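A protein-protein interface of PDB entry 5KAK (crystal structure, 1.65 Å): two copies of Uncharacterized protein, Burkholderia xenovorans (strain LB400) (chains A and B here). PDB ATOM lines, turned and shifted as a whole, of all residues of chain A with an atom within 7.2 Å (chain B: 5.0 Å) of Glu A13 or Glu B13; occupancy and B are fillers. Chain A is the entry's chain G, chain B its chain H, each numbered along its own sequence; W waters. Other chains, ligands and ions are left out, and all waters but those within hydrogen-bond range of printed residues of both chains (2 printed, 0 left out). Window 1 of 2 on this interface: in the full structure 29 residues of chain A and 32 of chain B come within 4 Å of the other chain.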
ATOM      1  N   VAL A  11     -23.443 -16.975  11.611  1.00  0.00           N
ATOM      2  CA  VAL A  11     -22.778 -18.267  11.487  1.00  0.00           C
ATOM      3  C   VAL A  11     -22.046 -18.290  10.158  1.00  0.00           C
ATOM      4  O   VAL A  11     -22.639 -17.995   9.116  1.00  0.00           O
ATOM      5  CB  VAL A  11     -23.768 -19.442  11.590  1.00  0.00           C
ATOM      6  CG1 VAL A  11     -23.064 -20.750  11.307  1.00  0.00           C
ATOM      7  CG2 VAL A  11     -24.423 -19.461  12.973  1.00  0.00           C
ATOM      8  N   GLU A  12     -20.749 -18.579  10.206  1.00  0.00           N
ATOM      9  CA  GLU A  12     -19.971 -18.811   9.006  1.00  0.00           C
ATOM     10  C   GLU A  12     -19.934 -20.299   8.713  1.00  0.00           C
ATOM     11  O   GLU A  12     -19.551 -21.107   9.572  1.00  0.00           O
ATOM     12  CB  GLU A  12     -18.539 -18.292   9.163  1.00  0.00           C
ATOM     13  CG  GLU A  12     -17.691 -18.588   7.937  1.00  0.00           C
ATOM     14  CD  GLU A  12     -16.241 -18.148   8.076  1.00  0.00           C
ATOM     15  OE1 GLU A  12     -15.792 -17.817   9.193  1.00  0.00           O
ATOM     16  OE2 GLU A  12     -15.537 -18.125   7.050  1.00  0.00           O
ATOM     17  N   GLU A  13     -20.278 -20.664   7.491  1.00  0.00           N
ATOM     18  CA  GLU A  13     -20.093 -22.031   7.031  1.00  0.00           C
ATOM     19  C   GLU A  13     -18.896 -22.054   6.099  1.00  0.00           C
ATOM     20  O   GLU A  13     -18.870 -21.334   5.096  1.00  0.00           O
ATOM     21  CB  GLU A  13     -21.339 -22.572   6.334  1.00  0.00           C
ATOM     22  CG  GLU A  13     -21.187 -24.013   5.919  1.00  0.00           C
ATOM     23  CD  GLU A  13     -22.485 -24.595   5.381  1.00  0.00           C
ATOM     24  OE1 GLU A  13     -23.378 -23.817   4.978  1.00  0.00           O
ATOM     25  OE2 GLU A  13     -22.612 -25.831   5.359  1.00  0.00           O
ATOM     26  N   ARG A  14     -17.896 -22.851   6.451  1.00  0.00           N
ATOM     27  CA  ARG A  14     -16.735 -23.055   5.603  1.00  0.00           C
ATOM     28  C   ARG A  14     -16.800 -24.453   5.009  1.00  0.00           C
ATOM     29  O   ARG A  14     -17.141 -25.418   5.692  1.00  0.00           O
ATOM     30  CB  ARG A  14     -15.446 -22.838   6.379  1.00  0.00           C
ATOM     31  CG  ARG A  14     -15.324 -21.383   6.803  1.00  0.00           C
ATOM     32  CD  ARG A  14     -14.109 -21.113   7.672  1.00  0.00           C
ATOM     33  NE  ARG A  14     -12.849 -21.083   6.924  1.00  0.00           N
ATOM     34  CZ  ARG A  14     -12.424 -20.059   6.191  1.00  0.00           C
ATOM     35  NH1 ARG A  14     -13.173 -18.973   6.050  1.00  0.00           N
ATOM     36  NH2 ARG A  14     -11.251 -20.133   5.581  1.00  0.00           N
ATOM     37  N   ILE A  15     -16.472 -24.542   3.730  1.00  0.00           N
ATOM     38  CA  ILE A  15     -16.629 -25.750   2.944  1.00  0.00           C
ATOM     39  C   ILE A  15     -15.304 -25.969   2.234  1.00  0.00           C
ATOM     40  O   ILE A  15     -14.943 -25.194   1.339  1.00  0.00           O
ATOM     41  CB  ILE A  15     -17.769 -25.619   1.932  1.00  0.00           C
ATOM     42  CG1 ILE A  15     -19.074 -25.264   2.642  1.00  0.00           C
ATOM     43  CG2 ILE A  15     -17.904 -26.889   1.108  1.00  0.00           C
ATOM     44  CD1 ILE A  15     -20.293 -25.207   1.672  1.00  0.00           C
ATOM     45  N   PHE A  49     -17.702 -31.429  10.296  1.00  0.00           N
ATOM     46  CA  PHE A  49     -18.164 -32.649   9.658  1.00  0.00           C
ATOM     47  C   PHE A  49     -17.308 -32.972   8.447  1.00  0.00           C
ATOM     48  O   PHE A  49     -16.588 -32.118   7.915  1.00  0.00           O
ATOM     49  CB  PHE A  49     -19.629 -32.531   9.176  1.00  0.00           C
ATOM     50  CG  PHE A  49     -20.568 -31.964  10.198  1.00  0.00           C
ATOM     51  CD1 PHE A  49     -21.110 -32.769  11.192  1.00  0.00           C
ATOM     52  CD2 PHE A  49     -20.942 -30.628  10.147  1.00  0.00           C
ATOM     53  CE1 PHE A  49     -21.984 -32.241  12.129  1.00  0.00           C
ATOM     54  CE2 PHE A  49     -21.832 -30.101  11.070  1.00  0.00           C
ATOM     55  CZ  PHE A  49     -22.346 -30.906  12.065  1.00  0.00           C
ATOM     56  N   THR A  51     -18.166 -35.194   4.632  1.00  0.00           N
ATOM     57  CA  THR A  51     -19.292 -35.714   3.878  1.00  0.00           C
ATOM     58  C   THR A  51     -19.183 -37.224   3.760  1.00  0.00           C
ATOM     59  O   THR A  51     -18.080 -37.786   3.670  1.00  0.00           O
ATOM     60  CB  THR A  51     -19.376 -35.088   2.477  1.00  0.00           C
ATOM     61  OG1 THR A  51     -18.123 -35.243   1.789  1.00  0.00           O
ATOM     62  CG2 THR A  51     -19.724 -33.613   2.580  1.00  0.00           C
ATOM     63  N   GLN A  58     -14.966 -33.919   1.439  1.00  0.00           N
ATOM     64  CA  GLN A  58     -15.321 -32.554   1.778  1.00  0.00           C
ATOM     65  C   GLN A  58     -15.490 -32.453   3.274  1.00  0.00           C
ATOM     66  O   GLN A  58     -16.079 -33.341   3.898  1.00  0.00           O
ATOM     67  CB  GLN A  58     -16.626 -32.126   1.095  1.00  0.00           C
ATOM     68  CG  GLN A  58     -16.939 -30.667   1.172  1.00  0.00           C
ATOM     69  CD  GLN A  58     -18.245 -30.321   0.475  1.00  0.00           C
ATOM     70  OE1 GLN A  58     -19.334 -30.425   1.060  1.00  0.00           O
ATOM     71  NE2 GLN A  58     -18.142 -29.888  -0.778  1.00  0.00           N
ATOM     72  N   VAL A  60     -16.933 -29.722   6.298  1.00  0.00           N
ATOM     73  CA  VAL A  60     -17.897 -28.637   6.455  1.00  0.00           C
ATOM     74  C   VAL A  60     -17.862 -28.241   7.914  1.00  0.00           C
ATOM     75  O   VAL A  60     -18.016 -29.102   8.788  1.00  0.00           O
ATOM     76  CB  VAL A  60     -19.322 -29.078   6.068  1.00  0.00           C
ATOM     77  CG1 VAL A  60     -20.324 -28.002   6.426  1.00  0.00           C
ATOM     78  CG2 VAL A  60     -19.401 -29.455   4.591  1.00  0.00           C
ATOM     79  N   HIS A  61     -17.668 -26.955   8.184  1.00  0.00           N
ATOM     80  CA  HIS A  61     -17.589 -26.526   9.571  1.00  0.00           C
ATOM     81  C   HIS A  61     -18.295 -25.193   9.731  1.00  0.00           C
ATOM     82  O   HIS A  61     -18.248 -24.333   8.847  1.00  0.00           O
ATOM     83  CB  HIS A  61     -16.133 -26.486  10.116  1.00  0.00           C
ATOM     84  CG  HIS A  61     -15.087 -25.969   9.166  1.00  0.00           C
ATOM     85  ND1 HIS A  61     -14.274 -24.909   9.493  1.00  0.00           N
ATOM     86  CD2 HIS A  61     -14.649 -26.419   7.965  1.00  0.00           C
ATOM     87  CE1 HIS A  61     -13.413 -24.690   8.517  1.00  0.00           C
ATOM     88  NE2 HIS A  61     -13.618 -25.595   7.574  1.00  0.00           N
ATOM     89  N   LEU A  62     -19.014 -25.069  10.838  1.00  0.00           N
ATOM     90  CA  LEU A  62     -19.888 -23.935  11.090  1.00  0.00           C
ATOM     91  C   LEU A  62     -19.402 -23.263  12.359  1.00  0.00           C
ATOM     92  O   LEU A  62     -19.224 -23.927  13.377  1.00  0.00           O
ATOM     93  CB  LEU A  62     -21.358 -24.386  11.218  1.00  0.00           C
ATOM     94  CG  LEU A  62     -21.973 -24.872   9.878  1.00  0.00           C
ATOM     95  CD1 LEU A  62     -21.595 -26.292   9.556  1.00  0.00           C
ATOM     96  CD2 LEU A  62     -23.490 -24.702   9.838  1.00  0.00           C
ATOM     97  N   TRP A  63     -19.141 -21.965  12.277  1.00  0.00           N
ATOM     98  CA  TRP A  63     -18.579 -21.203  13.384  1.00  0.00           C
ATOM     99  C   TRP A  63     -19.525 -20.065  13.726  1.00  0.00           C
ATOM    100  O   TRP A  63     -19.938 -19.310  12.847  1.00  0.00           O
ATOM    101  CB  TRP A  63     -17.197 -20.665  13.011  1.00  0.00           C
ATOM    102  CG  TRP A  63     -16.194 -21.756  12.763  1.00  0.00           C
ATOM    103  CD1 TRP A  63     -15.938 -22.395  11.570  1.00  0.00           C
ATOM    104  CD2 TRP A  63     -15.335 -22.356  13.734  1.00  0.00           C
ATOM    105  NE1 TRP A  63     -14.957 -23.347  11.748  1.00  0.00           N
ATOM    106  CE2 TRP A  63     -14.569 -23.334  13.067  1.00  0.00           C
ATOM    107  CE3 TRP A  63     -15.127 -22.148  15.113  1.00  0.00           C
ATOM    108  CZ2 TRP A  63     -13.615 -24.115  13.726  1.00  0.00           C
ATOM    109  CZ3 TRP A  63     -14.169 -22.928  15.766  1.00  0.00           C
ATOM    110  CH2 TRP A  63     -13.437 -23.901  15.066  1.00  0.00           C
ATOM    111  N   GLN A 100     -14.341 -22.479   0.169  1.00  0.00           N
ATOM    112  CA  GLN A 100     -15.364 -21.453   0.018  1.00  0.00           C
ATOM    113  C   GLN A 100     -16.048 -21.252   1.363  1.00  0.00           C
ATOM    114  O   GLN A 100     -16.024 -22.133   2.228  1.00  0.00           O
ATOM    115  CB  GLN A 100     -16.389 -21.822  -1.053  1.00  0.00           C
ATOM    116  CG  GLN A 100     -17.094 -23.132  -0.822  1.00  0.00           C
ATOM    117  CD  GLN A 100     -17.863 -23.567  -2.048  1.00  0.00           C
ATOM    118  OE1 GLN A 100     -17.411 -24.420  -2.815  1.00  0.00           O
ATOM    119  NE2 GLN A 100     -19.020 -22.963  -2.254  1.00  0.00           N
ATOM    120  N   ASN A 101     -16.648 -20.073   1.548  1.00  0.00           N
ATOM    121  CA  ASN A 101     -17.439 -19.839   2.751  1.00  0.00           C
ATOM    122  C   ASN A 101     -18.670 -18.998   2.435  1.00  0.00           C
ATOM    123  O   ASN A 101     -18.755 -18.353   1.392  1.00  0.00           O
ATOM    124  CB  ASN A 101     -16.609 -19.166   3.848  1.00  0.00           C
ATOM    125  CG  ASN A 101     -16.045 -17.820   3.413  1.00  0.00           C
ATOM    126  OD1 ASN A 101     -16.003 -17.518   2.246  1.00  0.00           O
ATOM    127  ND2 ASN A 101     -15.606 -17.009   4.371  1.00  0.00           N
ATOM    128  N   LYS A 102     -19.631 -19.040   3.365  1.00  0.00           N
ATOM    129  CA  LYS A 102     -20.855 -18.252   3.318  1.00  0.00           C
ATOM    130  C   LYS A 102     -21.191 -17.760   4.726  1.00  0.00           C
ATOM    131  O   LYS A 102     -20.790 -18.355   5.735  1.00  0.00           O
ATOM    132  CB  LYS A 102     -22.030 -19.045   2.704  1.00  0.00           C
ATOM    133  CG  LYS A 102     -22.375 -20.364   3.372  1.00  0.00           C
ATOM    134  CD  LYS A 102     -23.571 -21.105   2.710  1.00  0.00           C
ATOM    135  CE  LYS A 102     -23.251 -21.727   1.361  1.00  0.00           C
ATOM    136  NZ  LYS A 102     -24.276 -22.766   0.975  1.00  0.00           N
ATOM    137  N   ILE A 103     -21.914 -16.654   4.792  1.00  0.00           N
ATOM    138  CA  ILE A 103     -22.416 -16.147   6.060  1.00  0.00           C
ATOM    139  C   ILE A 103     -23.905 -16.481   6.132  1.00  0.00           C
ATOM    140  O   ILE A 103     -24.673 -16.112   5.238  1.00  0.00           O
ATOM    141  CB  ILE A 103     -22.141 -14.641   6.222  1.00  0.00           C
ATOM    142  CG1 ILE A 103     -20.633 -14.357   6.179  1.00  0.00           C
ATOM    143  CG2 ILE A 103     -22.660 -14.134   7.558  1.00  0.00           C
ATOM    144  CD1 ILE A 103     -19.850 -15.138   7.215  1.00  0.00           C
ATOM    145  N   LEU A 104     -24.283 -17.201   7.192  1.00  0.00           N
ATOM    146  CA  LEU A 104     -25.635 -17.666   7.488  1.00  0.00           C
ATOM    147  C   LEU A 104     -26.246 -16.873   8.635  1.00  0.00           C
ATOM    148  O   LEU A 104     -25.576 -16.593   9.621  1.00  0.00           O
ATOM    149  CB  LEU A 104     -25.621 -19.144   7.876  1.00  0.00           C
ATOM    150  CG  LEU A 104     -25.016 -20.091   6.829  1.00  0.00           C
ATOM    151  CD1 LEU A 104     -25.131 -21.542   7.247  1.00  0.00           C
ATOM    152  CD2 LEU A 104     -25.645 -19.867   5.457  1.00  0.00           C
ATOM    153  N   VAL B  11     -25.657 -36.209  10.372  1.00  0.00           N
ATOM    154  CA  VAL B  11     -26.290 -34.912  10.196  1.00  0.00           C
ATOM    155  C   VAL B  11     -26.640 -34.744   8.724  1.00  0.00           C
ATOM    156  O   VAL B  11     -25.790 -34.947   7.853  1.00  0.00           O
ATOM    157  CB  VAL B  11     -25.387 -33.762  10.675  1.00  0.00           C
ATOM    158  CG1 VAL B  11     -25.996 -32.432  10.303  1.00  0.00           C
ATOM    159  CG2 VAL B  11     -25.213 -33.835  12.172  1.00  0.00           C
ATOM    160  N   GLU B  12     -27.893 -34.398   8.452  1.00  0.00           N
ATOM    161  CA  GLU B  12     -28.336 -34.090   7.101  1.00  0.00           C
ATOM    162  C   GLU B  12     -28.326 -32.582   6.945  1.00  0.00           C
ATOM    163  O   GLU B  12     -28.961 -31.873   7.735  1.00  0.00           O
ATOM    164  CB  GLU B  12     -29.735 -34.638   6.811  1.00  0.00           C
ATOM    165  CG  GLU B  12     -30.198 -34.219   5.414  1.00  0.00           C
ATOM    166  CD  GLU B  12     -31.590 -34.702   5.089  1.00  0.00           C
ATOM    167  OE1 GLU B  12     -32.276 -35.186   6.010  1.00  0.00           O
ATOM    168  OE2 GLU B  12     -32.000 -34.588   3.909  1.00  0.00           O
ATOM    169  N   GLU B  13     -27.582 -32.093   5.963  1.00  0.00           N
ATOM    170  CA  GLU B  13     -27.640 -30.693   5.594  1.00  0.00           C
ATOM    171  C   GLU B  13     -28.541 -30.560   4.370  1.00  0.00           C
ATOM    172  O   GLU B  13     -28.363 -31.284   3.381  1.00  0.00           O
ATOM    173  CB  GLU B  13     -26.252 -30.130   5.303  1.00  0.00           C
ATOM    174  CG  GLU B  13     -26.317 -28.694   4.842  1.00  0.00           C
ATOM    175  CD  GLU B  13     -24.963 -28.046   4.813  1.00  0.00           C
ATOM    176  OE1 GLU B  13     -23.959 -28.748   4.554  1.00  0.00           O
ATOM    177  OE2 GLU B  13     -24.912 -26.836   5.097  1.00  0.00           O
ATOM    178  N   ARG B  14     -29.540 -29.694   4.464  1.00  0.00           N
ATOM    179  CA  ARG B  14     -30.437 -29.431   3.340  1.00  0.00           C
ATOM    180  C   ARG B  14     -30.265 -27.988   2.867  1.00  0.00           C
ATOM    181  O   ARG B  14     -30.198 -27.057   3.679  1.00  0.00           O
ATOM    182  CB  ARG B  14     -31.883 -29.750   3.730  1.00  0.00           C
ATOM    183  CG  ARG B  14     -32.079 -31.271   3.978  1.00  0.00           C
ATOM    184  CD  ARG B  14     -33.511 -31.686   4.358  1.00  0.00           C
ATOM    185  NE  ARG B  14     -34.444 -31.508   3.247  1.00  0.00           N
ATOM    186  CZ  ARG B  14     -34.640 -32.387   2.269  1.00  0.00           C
ATOM    187  NH1 ARG B  14     -33.966 -33.527   2.246  1.00  0.00           N
ATOM    188  NH2 ARG B  14     -35.521 -32.113   1.310  1.00  0.00           N
ATOM    189  N   ILE B  15     -30.168 -27.804   1.556  1.00  0.00           N
ATOM    190  CA  ILE B  15     -29.788 -26.515   0.963  1.00  0.00           C
ATOM    191  C   ILE B  15     -30.827 -26.142  -0.094  1.00  0.00           C
ATOM    192  O   ILE B  15     -30.935 -26.809  -1.133  1.00  0.00           O
ATOM    193  CB  ILE B  15     -28.385 -26.560   0.348  1.00  0.00           C
ATOM    194  CG1 ILE B  15     -27.320 -26.883   1.416  1.00  0.00           C
ATOM    195  CG2 ILE B  15     -28.102 -25.262  -0.411  1.00  0.00           C
ATOM    196  CD1 ILE B  15     -25.970 -27.222   0.822  1.00  0.00           C
ATOM    197  N   VAL B  60     -30.479 -22.824   4.549  1.00  0.00           N
ATOM    198  CA  VAL B  60     -29.586 -23.923   4.893  1.00  0.00           C
ATOM    199  C   VAL B  60     -30.060 -24.460   6.227  1.00  0.00           C
ATOM    200  O   VAL B  60     -30.150 -23.702   7.204  1.00  0.00           O
ATOM    201  CB  VAL B  60     -28.113 -23.486   4.973  1.00  0.00           C
ATOM    202  CG1 VAL B  60     -27.211 -24.675   5.344  1.00  0.00           C
ATOM    203  CG2 VAL B  60     -27.680 -22.822   3.677  1.00  0.00           C
ATOM    204  N   HIS B  61     -30.378 -25.745   6.276  1.00  0.00           N
ATOM    205  CA  HIS B  61     -30.778 -26.307   7.557  1.00  0.00           C
ATOM    206  C   HIS B  61     -30.119 -27.654   7.806  1.00  0.00           C
ATOM    207  O   HIS B  61     -29.910 -28.457   6.884  1.00  0.00           O
ATOM    208  CB  HIS B  61     -32.319 -26.402   7.698  1.00  0.00           C
ATOM    209  CG  HIS B  61     -33.054 -26.882   6.482  1.00  0.00           C
ATOM    210  ND1 HIS B  61     -33.902 -27.966   6.527  1.00  0.00           N
ATOM    211  CD2 HIS B  61     -33.170 -26.362   5.239  1.00  0.00           C
ATOM    212  CE1 HIS B  61     -34.466 -28.128   5.344  1.00  0.00           C
ATOM    213  NE2 HIS B  61     -34.039 -27.165   4.544  1.00  0.00           N
ATOM    214  N   LEU B  62     -29.757 -27.882   9.064  1.00  0.00           N
ATOM    215  CA  LEU B  62     -29.013 -29.075   9.446  1.00  0.00           C
ATOM    216  C   LEU B  62     -29.790 -29.833  10.509  1.00  0.00           C
ATOM    217  O   LEU B  62     -30.179 -29.254  11.532  1.00  0.00           O
ATOM    218  CB  LEU B  62     -27.613 -28.729   9.964  1.00  0.00           C
ATOM    219  CG  LEU B  62     -26.627 -28.256   8.903  1.00  0.00           C
ATOM    220  CD1 LEU B  62     -26.745 -26.754   8.663  1.00  0.00           C
ATOM    221  CD2 LEU B  62     -25.214 -28.641   9.279  1.00  0.00           C
ATOM    222  N   GLN B 100     -31.020 -29.427  -2.668  1.00  0.00           N
ATOM    223  CA  GLN B 100     -29.930 -30.388  -2.556  1.00  0.00           C
ATOM    224  C   GLN B 100     -29.786 -30.791  -1.100  1.00  0.00           C
ATOM    225  O   GLN B 100     -30.120 -30.023  -0.194  1.00  0.00           O
ATOM    226  CB  GLN B 100     -28.571 -29.829  -2.992  1.00  0.00           C
ATOM    227  CG  GLN B 100     -28.555 -29.054  -4.282  1.00  0.00           C
ATOM    228  CD  GLN B 100     -27.272 -28.267  -4.437  1.00  0.00           C
ATOM    229  OE1 GLN B 100     -26.199 -28.833  -4.662  1.00  0.00           O
ATOM    230  NE2 GLN B 100     -27.369 -26.956  -4.295  1.00  0.00           N
ATOM    231  N   ASN B 101     -29.259 -31.995  -0.867  1.00  0.00           N
ATOM    232  CA  ASN B 101     -28.908 -32.372   0.495  1.00  0.00           C
ATOM    233  C   ASN B 101     -27.611 -33.172   0.495  1.00  0.00           C
ATOM    234  O   ASN B 101     -27.124 -33.624  -0.544  1.00  0.00           O
ATOM    235  CB  ASN B 101     -30.058 -33.125   1.195  1.00  0.00           C
ATOM    236  CG  ASN B 101     -30.375 -34.453   0.555  1.00  0.00           C
ATOM    237  OD1 ASN B 101     -30.034 -34.698  -0.594  1.00  0.00           O
ATOM    238  ND2 ASN B 101     -31.031 -35.336   1.314  1.00  0.00           N
ATOM    239  N   LYS B 102     -27.024 -33.277   1.686  1.00  0.00           N
ATOM    240  CA  LYS B 102     -25.804 -34.036   1.936  1.00  0.00           C
ATOM    241  C   LYS B 102     -25.978 -34.782   3.250  1.00  0.00           C
ATOM    242  O   LYS B 102     -26.750 -34.365   4.116  1.00  0.00           O
ATOM    243  CB  LYS B 102     -24.543 -33.153   2.062  1.00  0.00           C
ATOM    244  CG  LYS B 102     -24.386 -31.988   1.104  1.00  0.00           C
ATOM    245  CD  LYS B 102     -23.180 -31.155   1.515  1.00  0.00           C
ATOM    246  CE  LYS B 102     -22.888 -30.046   0.536  1.00  0.00           C
ATOM    247  NZ  LYS B 102     -21.590 -29.371   0.836  1.00  0.00           N
ATOM    248  N   LEU B 104     -23.666 -35.630   6.427  1.00  0.00           N
ATOM    249  CA  LEU B 104     -22.444 -35.205   7.096  1.00  0.00           C
ATOM    250  C   LEU B 104     -22.194 -36.076   8.322  1.00  0.00           C
ATOM    251  O   LEU B 104     -23.128 -36.425   9.047  1.00  0.00           O
ATOM    252  CB  LEU B 104     -22.557 -33.741   7.525  1.00  0.00           C
ATOM    253  CG  LEU B 104     -22.955 -32.711   6.465  1.00  0.00           C
ATOM    254  CD1 LEU B 104     -22.922 -31.328   7.102  1.00  0.00           C
ATOM    255  CD2 LEU B 104     -21.994 -32.761   5.292  1.00  0.00           C
HETATM  256  O   HOH W   1     -24.454 -24.866   2.664  1.00  0.00           O
HETATM  257  O   HOH W   2     -22.153 -27.594   2.972  1.00  0.00           O
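The side-chain carboxylate of Glu A13 lies close to the side-chain carboxylate of Glu B13 (2.5 Å).
The side-chain amino group (NZ) of Lys B102 is in hydrogen-bond range of the side-chain amide oxygen (OE1) of Gln A58, 2.5 Å away.
O of Val B11 sits at hydrogen-bond distance from N of Leu B104 (2.6 Å).
O of Val A60 sits at hydrogen-bond distance from N of Phe A49 (2.8 Å).
N of Glu A13 sits at hydrogen-bond distance from O of Lys A102 (2.9 Å).
O of Glu B13 sits at hydrogen-bond distance from N of Lys B102 (2.9 Å).
The backbone NH (N) of Thr A51 sits at hydrogen-bond distance from the backbone carbonyl oxygen (O) of Gln A58, at 2.9 Å.
Val B60 touches Glu A13.
CE1 of Phe A49 touches CG2 of Val B11, 3.6 Å away.
Leu B104 touches Phe A49.
CG2 of Thr A51 touches CD2 of Leu B104, 3.6 Å away.
Glu A13 touches two residues of chain B.
Of the printed residues of chain B, Phe A49 touches Val B11 and Leu B104.
Of the printed residues of chain B, Gln A58 touches Lys B102 (2.5 Å).
Glu B13 touches just one residue of chain A: Glu A13 (2.5 Å).
Printed residues of chain A within 4 Å of Leu B104: Phe A49 and Thr A51.
The nearest residue of chain A that does not touch Glu B13 is Val A60 (4.2 Å).
The nearest printed residue of chain B that does not touch Thr A51 is Lys B102 (4.4 Å).
Of the 12 printed residues of chain B, 5 touch a printed residue of chain A.
Printed residues of chain B that touch a printed residue of chain A: Val B11, Glu B13, Val B60, Lys B102 and Leu B104.
Hydrophobic or aromatic side chains of chain B within 4 Å of the printed part of chain A: Val B11, Val B60 and Leu B104.
Along chain B the printed residues that touch a printed residue of chain A span positions 11 to 104.
Hydrophobic or aromatic side chains of chain A that line the printed part of chain B: Phe A49.
Glu A13 touches its own counterpart, Glu B13.
Glu A13 touches Val B60, but with the chains exchanged Val A60 does not touch Glu B13 (4.2 Å).
Positions printed for both chains: 11, 12, 13, 14, 15, 60, 61, 62, 100, 101, 102 and 104.
Of the 6 pairs that touch across the chains among the printed residues, 1 has its exchanged pair printed and touching as well.
Water W2 lies within hydrogen-bond range of the side-chain carboxylate of Glu B13 (2.7 Å), the side-chain amino group of Lys B102 (2.8 Å) and the side-chain carboxylate of Glu A13 (3.0 Å).
Water W1 lies within hydrogen-bond range of NZ of Lys A102, OE1 of Glu A13 and OE2 of Glu B13.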
